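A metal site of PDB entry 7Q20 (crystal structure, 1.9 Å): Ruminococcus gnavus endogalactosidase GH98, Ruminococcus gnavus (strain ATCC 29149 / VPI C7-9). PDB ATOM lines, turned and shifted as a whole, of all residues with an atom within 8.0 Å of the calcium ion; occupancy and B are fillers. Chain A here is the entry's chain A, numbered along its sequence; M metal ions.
The backbone NH (N) of Met 207 sits at hydrogen-bond distance from the backbone carbonyl oxygen (O) of Lys 89. The backbone NH of Lys 89 sits at hydrogen-bond distance from the backbone carbonyl oxygen of Glu 208 (2.9 Å). The backbone NH of Gly 33 lies within hydrogen-bond range of the side-chain carboxylate of Glu 208 (2.8 Å). OD1 of Asp 34 is in hydrogen-bond range of N of Tyr 36 (3.1 Å).
Within 4 Å of the calcium ion: Leu 29, Asp 32, Asp 34, Tyr 37, Met 207 and Glu 208. The nearest printed residue that does not touch the calcium ion is Leu 30 (4.5 Å).
OD1 of Asp 32 binds the calcium ion, 2.2 Å away. O of Met 207 binds the calcium ion, at 2.2 Å. The side-chain carboxylate (OE1) of Glu 208 is bound to the calcium ion (2.3 Å). The calcium ion is bound by O of Asp 34 (2.3 Å). The calcium ion is bound by O of Leu 29 (2.4 Å). The calcium ion is bound by OH of Tyr 37, at 2.4 Å.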
ATOM      1  N   ASN A  26       5.993 -17.772  -0.384  1.00  0.00           N
ATOM      2  CA  ASN A  26       4.664 -17.800   0.207  1.00  0.00           C
ATOM      3  C   ASN A  26       3.519 -17.877  -0.822  1.00  0.00           C
ATOM      4  O   ASN A  26       2.645 -17.027  -0.891  1.00  0.00           O
ATOM      5  CB  ASN A  26       4.490 -16.637   1.176  1.00  0.00           C
ATOM      6  CG  ASN A  26       5.361 -16.780   2.410  1.00  0.00           C
ATOM      7  OD1 ASN A  26       5.922 -15.796   2.920  1.00  0.00           O
ATOM      8  ND2 ASN A  26       5.490 -18.004   2.914  1.00  0.00           N
ATOM      9  N   ALA A  27       3.594 -18.953  -1.622  1.00  0.00           N
ATOM     10  CA  ALA A  27       2.632 -19.266  -2.666  1.00  0.00           C
ATOM     11  C   ALA A  27       1.157 -19.301  -2.216  1.00  0.00           C
ATOM     12  O   ALA A  27       0.241 -18.938  -2.989  1.00  0.00           O
ATOM     13  CB  ALA A  27       2.995 -20.593  -3.307  1.00  0.00           C
ATOM     14  N   ASP A  28       0.918 -19.754  -0.981  1.00  0.00           N
ATOM     15  CA  ASP A  28      -0.456 -19.911  -0.454  1.00  0.00           C
ATOM     16  C   ASP A  28      -1.230 -18.613  -0.316  1.00  0.00           C
ATOM     17  O   ASP A  28      -2.456 -18.639  -0.280  1.00  0.00           O
ATOM     18  CB  ASP A  28      -0.436 -20.647   0.875  1.00  0.00           C
ATOM     19  CG  ASP A  28       0.048 -22.083   0.728  1.00  0.00           C
ATOM     20  OD1 ASP A  28      -0.560 -22.845  -0.035  1.00  0.00           O
ATOM     21  OD2 ASP A  28       1.055 -22.468   1.370  1.00  0.00           O
ATOM     22  N   LEU A  29      -0.509 -17.490  -0.218  1.00  0.00           N
ATOM     23  CA  LEU A  29      -1.128 -16.184  -0.112  1.00  0.00           C
ATOM     24  C   LEU A  29      -1.882 -15.776  -1.401  1.00  0.00           C
ATOM     25  O   LEU A  29      -2.818 -14.993  -1.335  1.00  0.00           O
ATOM     26  CB  LEU A  29      -0.105 -15.112   0.305  1.00  0.00           C
ATOM     27  CG  LEU A  29       0.590 -15.347   1.657  1.00  0.00           C
ATOM     28  CD1 LEU A  29       1.636 -14.270   1.935  1.00  0.00           C
ATOM     29  CD2 LEU A  29      -0.407 -15.432   2.803  1.00  0.00           C
ATOM     30  N   LEU A  30      -1.495 -16.347  -2.549  1.00  0.00           N
ATOM     31  CA  LEU A  30      -2.107 -16.027  -3.844  1.00  0.00           C
ATOM     32  C   LEU A  30      -3.601 -16.363  -3.911  1.00  0.00           C
ATOM     33  O   LEU A  30      -4.398 -15.669  -4.568  1.00  0.00           O
ATOM     34  CB  LEU A  30      -1.342 -16.757  -4.969  1.00  0.00           C
ATOM     35  CG  LEU A  30      -1.663 -16.373  -6.407  1.00  0.00           C
ATOM     36  CD1 LEU A  30      -1.252 -14.937  -6.680  1.00  0.00           C
ATOM     37  CD2 LEU A  30      -1.011 -17.319  -7.382  1.00  0.00           C
ATOM     38  N   THR A  31      -3.987 -17.454  -3.233  1.00  0.00           N
ATOM     39  CA  THR A  31      -5.306 -18.037  -3.364  1.00  0.00           C
ATOM     40  C   THR A  31      -6.000 -18.259  -2.021  1.00  0.00           C
ATOM     41  O   THR A  31      -6.798 -19.169  -1.888  1.00  0.00           O
ATOM     42  CB  THR A  31      -5.224 -19.352  -4.166  1.00  0.00           C
ATOM     43  OG1 THR A  31      -4.496 -20.341  -3.425  1.00  0.00           O
ATOM     44  CG2 THR A  31      -4.527 -19.121  -5.505  1.00  0.00           C
ATOM     45  N   ASP A  32      -5.730 -17.380  -1.051  1.00  0.00           N
ATOM     46  CA  ASP A  32      -6.288 -17.493   0.302  1.00  0.00           C
ATOM     47  C   ASP A  32      -7.605 -16.730   0.530  1.00  0.00           C
ATOM     48  O   ASP A  32      -8.130 -16.745   1.619  1.00  0.00           O
ATOM     49  CB  ASP A  32      -5.216 -17.136   1.373  1.00  0.00           C
ATOM     50  CG  ASP A  32      -4.719 -15.673   1.294  1.00  0.00           C
ATOM     51  OD1 ASP A  32      -5.218 -14.865   0.450  1.00  0.00           O
ATOM     52  OD2 ASP A  32      -3.795 -15.335   2.089  1.00  0.00           O
ATOM     53  N   GLY A  33      -8.130 -16.072  -0.506  1.00  0.00           N
ATOM     54  CA  GLY A  33      -9.372 -15.309  -0.420  1.00  0.00           C
ATOM     55  C   GLY A  33      -9.231 -13.985   0.317  1.00  0.00           C
ATOM     56  O   GLY A  33     -10.220 -13.294   0.562  1.00  0.00           O
ATOM     57  N   ASP A  34      -7.992 -13.620   0.683  1.00  0.00           N
ATOM     58  CA  ASP A  34      -7.732 -12.421   1.463  1.00  0.00           C
ATOM     59  C   ASP A  34      -6.975 -11.433   0.571  1.00  0.00           C
ATOM     60  O   ASP A  34      -5.847 -11.719   0.135  1.00  0.00           O
ATOM     61  CB  ASP A  34      -6.901 -12.790   2.701  1.00  0.00           C
ATOM     62  CG  ASP A  34      -6.839 -11.678   3.741  1.00  0.00           C
ATOM     63  OD1 ASP A  34      -7.276 -10.555   3.484  1.00  0.00           O
ATOM     64  OD2 ASP A  34      -6.345 -11.943   4.835  1.00  0.00           O
ATOM     65  N   LYS A  35      -7.565 -10.247   0.365  1.00  0.00           N
ATOM     66  CA  LYS A  35      -6.948  -9.137  -0.353  1.00  0.00           C
ATOM     67  C   LYS A  35      -6.462  -7.983   0.490  1.00  0.00           C
ATOM     68  O   LYS A  35      -5.874  -7.033  -0.035  1.00  0.00           O
ATOM     69  CB  LYS A  35      -7.941  -8.586  -1.381  1.00  0.00           C
ATOM     70  CG  LYS A  35      -8.272  -9.597  -2.450  1.00  0.00           C
ATOM     71  CD  LYS A  35      -8.987  -8.977  -3.650  1.00  0.00           C
ATOM     72  CE  LYS A  35     -10.359  -8.482  -3.360  1.00  0.00           C
ATOM     73  NZ  LYS A  35     -11.154  -8.249  -4.601  1.00  0.00           N
ATOM     74  N   TYR A  36      -6.706  -8.038   1.806  1.00  0.00           N
ATOM     75  CA  TYR A  36      -6.583  -6.878   2.735  1.00  0.00           C
ATOM     76  C   TYR A  36      -5.613  -7.163   3.908  1.00  0.00           C
ATOM     77  O   TYR A  36      -4.966  -6.213   4.347  1.00  0.00           O
ATOM     78  CB  TYR A  36      -7.987  -6.458   3.179  1.00  0.00           C
ATOM     79  CG  TYR A  36      -8.906  -6.288   2.000  1.00  0.00           C
ATOM     80  CD1 TYR A  36      -8.764  -5.229   1.129  1.00  0.00           C
ATOM     81  CD2 TYR A  36      -9.903  -7.224   1.725  1.00  0.00           C
ATOM     82  CE1 TYR A  36      -9.588  -5.084   0.014  1.00  0.00           C
ATOM     83  CE2 TYR A  36     -10.746  -7.081   0.631  1.00  0.00           C
ATOM     84  CZ  TYR A  36     -10.581  -6.022  -0.229  1.00  0.00           C
ATOM     85  OH  TYR A  36     -11.388  -5.899  -1.332  1.00  0.00           O
ATOM     86  N   TYR A  37      -5.528  -8.394   4.409  1.00  0.00           N
ATOM     87  CA  TYR A  37      -4.573  -8.835   5.473  1.00  0.00           C
ATOM     88  C   TYR A  37      -4.796  -7.994   6.742  1.00  0.00           C
ATOM     89  O   TYR A  37      -3.810  -7.543   7.377  1.00  0.00           O
ATOM     90  CB  TYR A  37      -3.143  -8.872   4.907  1.00  0.00           C
ATOM     91  CG  TYR A  37      -2.993  -9.987   3.894  1.00  0.00           C
ATOM     92  CD1 TYR A  37      -2.976 -11.309   4.315  1.00  0.00           C
ATOM     93  CD2 TYR A  37      -3.015  -9.735   2.536  1.00  0.00           C
ATOM     94  CE1 TYR A  37      -2.941 -12.357   3.397  1.00  0.00           C
ATOM     95  CE2 TYR A  37      -2.977 -10.766   1.603  1.00  0.00           C
ATOM     96  CZ  TYR A  37      -2.957 -12.084   2.037  1.00  0.00           C
ATOM     97  OH  TYR A  37      -2.922 -13.110   1.150  1.00  0.00           O
ATOM     98  N   GLN A  57       0.541  -7.897   2.182  1.00  0.00           N
ATOM     99  CA  GLN A  57       1.239  -9.172   2.131  1.00  0.00           C
ATOM    100  C   GLN A  57       0.852  -9.825   0.845  1.00  0.00           C
ATOM    101  O   GLN A  57      -0.157  -9.464   0.236  1.00  0.00           O
ATOM    102  CB  GLN A  57       0.808 -10.088   3.274  1.00  0.00           C
ATOM    103  CG  GLN A  57       0.787  -9.432   4.634  1.00  0.00           C
ATOM    104  CD  GLN A  57       2.154  -8.961   5.107  1.00  0.00           C
ATOM    105  OE1 GLN A  57       3.198  -9.240   4.503  1.00  0.00           O
ATOM    106  NE2 GLN A  57       2.138  -8.229   6.196  1.00  0.00           N
ATOM    107  N   GLY A  58       1.637 -10.827   0.419  1.00  0.00           N
ATOM    108  CA  GLY A  58       1.281 -11.560  -0.781  1.00  0.00           C
ATOM    109  C   GLY A  58       2.385 -12.438  -1.270  1.00  0.00           C
ATOM    110  O   GLY A  58       3.462 -12.449  -0.712  1.00  0.00           O
ATOM    111  N   THR A  59       2.073 -13.205  -2.312  1.00  0.00           N
ATOM    112  CA  THR A  59       3.021 -14.131  -2.916  1.00  0.00           C
ATOM    113  C   THR A  59       4.038 -13.289  -3.690  1.00  0.00           C
ATOM    114  O   THR A  59       3.679 -12.529  -4.557  1.00  0.00           O
ATOM    115  CB  THR A  59       2.309 -15.133  -3.810  1.00  0.00           C
ATOM    116  OG1 THR A  59       1.402 -15.924  -3.028  1.00  0.00           O
ATOM    117  CG2 THR A  59       3.317 -16.035  -4.491  1.00  0.00           C
ATOM    118  N   LYS A  89      -4.948  -8.856  -7.881  1.00  0.00           N
ATOM    119  CA  LYS A  89      -4.518  -7.744  -7.054  1.00  0.00           C
ATOM    120  C   LYS A  89      -3.064  -7.920  -6.702  1.00  0.00           C
ATOM    121  O   LYS A  89      -2.653  -8.958  -6.192  1.00  0.00           O
ATOM    122  CB  LYS A  89      -5.329  -7.639  -5.778  1.00  0.00           C
ATOM    123  CG  LYS A  89      -4.977  -6.367  -5.002  1.00  0.00           C
ATOM    124  CD  LYS A  89      -5.729  -6.222  -3.678  1.00  0.00           C
ATOM    125  CE  LYS A  89      -5.191  -5.033  -2.908  1.00  0.00           C
ATOM    126  NZ  LYS A  89      -5.845  -4.794  -1.590  1.00  0.00           N
ATOM    127  N   PHE A 206       2.064 -10.445  -5.428  1.00  0.00           N
ATOM    128  CA  PHE A 206       0.725 -10.790  -5.870  1.00  0.00           C
ATOM    129  C   PHE A 206      -0.138 -11.083  -4.630  1.00  0.00           C
ATOM    130  O   PHE A 206       0.040 -12.100  -3.955  1.00  0.00           O
ATOM    131  CB  PHE A 206       0.754 -12.025  -6.769  1.00  0.00           C
ATOM    132  CG  PHE A 206       1.497 -11.840  -8.062  1.00  0.00           C
ATOM    133  CD1 PHE A 206       0.865 -11.333  -9.192  1.00  0.00           C
ATOM    134  CD2 PHE A 206       2.826 -12.204  -8.167  1.00  0.00           C
ATOM    135  CE1 PHE A 206       1.557 -11.195 -10.385  1.00  0.00           C
ATOM    136  CE2 PHE A 206       3.517 -12.066  -9.360  1.00  0.00           C
ATOM    137  CZ  PHE A 206       2.889 -11.558 -10.468  1.00  0.00           C
ATOM    138  N   MET A 207      -1.054 -10.163  -4.312  1.00  0.00           N
ATOM    139  CA  MET A 207      -1.860 -10.273  -3.094  1.00  0.00           C
ATOM    140  C   MET A 207      -3.009 -11.292  -3.238  1.00  0.00           C
ATOM    141  O   MET A 207      -3.382 -11.989  -2.264  1.00  0.00           O
ATOM    142  CB  MET A 207      -2.378  -8.895  -2.700  1.00  0.00           C
ATOM    143  CG  MET A 207      -1.256  -7.926  -2.414  1.00  0.00           C
ATOM    144  SD  MET A 207      -1.818  -6.341  -1.770  1.00  0.00           S
ATOM    145  CE  MET A 207      -2.483  -6.841  -0.187  1.00  0.00           C
ATOM    146  N   GLU A 208      -3.560 -11.400  -4.454  1.00  0.00           N
ATOM    147  CA  GLU A 208      -4.626 -12.355  -4.735  1.00  0.00           C
ATOM    148  C   GLU A 208      -4.794 -12.565  -6.230  1.00  0.00           C
ATOM    149  O   GLU A 208      -4.634 -11.641  -7.006  1.00  0.00           O
ATOM    150  CB  GLU A 208      -5.942 -11.881  -4.140  1.00  0.00           C
ATOM    151  CG  GLU A 208      -7.124 -12.872  -4.130  1.00  0.00           C
ATOM    152  CD  GLU A 208      -6.954 -13.977  -3.100  1.00  0.00           C
ATOM    153  OE1 GLU A 208      -5.987 -13.922  -2.338  1.00  0.00           O
ATOM    154  OE2 GLU A 208      -7.777 -14.927  -3.070  1.00  0.00           O
ATOM    155  N   LEU A 209      -5.096 -13.814  -6.607  1.00  0.00           N
ATOM    156  CA  LEU A 209      -5.571 -14.168  -7.917  1.00  0.00           C
ATOM    157  C   LEU A 209      -6.801 -15.013  -7.704  1.00  0.00           C
ATOM    158  O   LEU A 209      -6.723 -16.187  -7.363  1.00  0.00           O
ATOM    159  CB  LEU A 209      -4.508 -14.936  -8.695  1.00  0.00           C
ATOM    160  CG  LEU A 209      -4.856 -15.252 -10.144  1.00  0.00           C
ATOM    161  CD1 LEU A 209      -5.138 -13.960 -10.908  1.00  0.00           C
ATOM    162  CD2 LEU A 209      -3.729 -16.031 -10.809  1.00  0.00           C
HETATM  163 CA    CA M   1      -4.392 -13.267  -0.795  1.00  0.00          CA
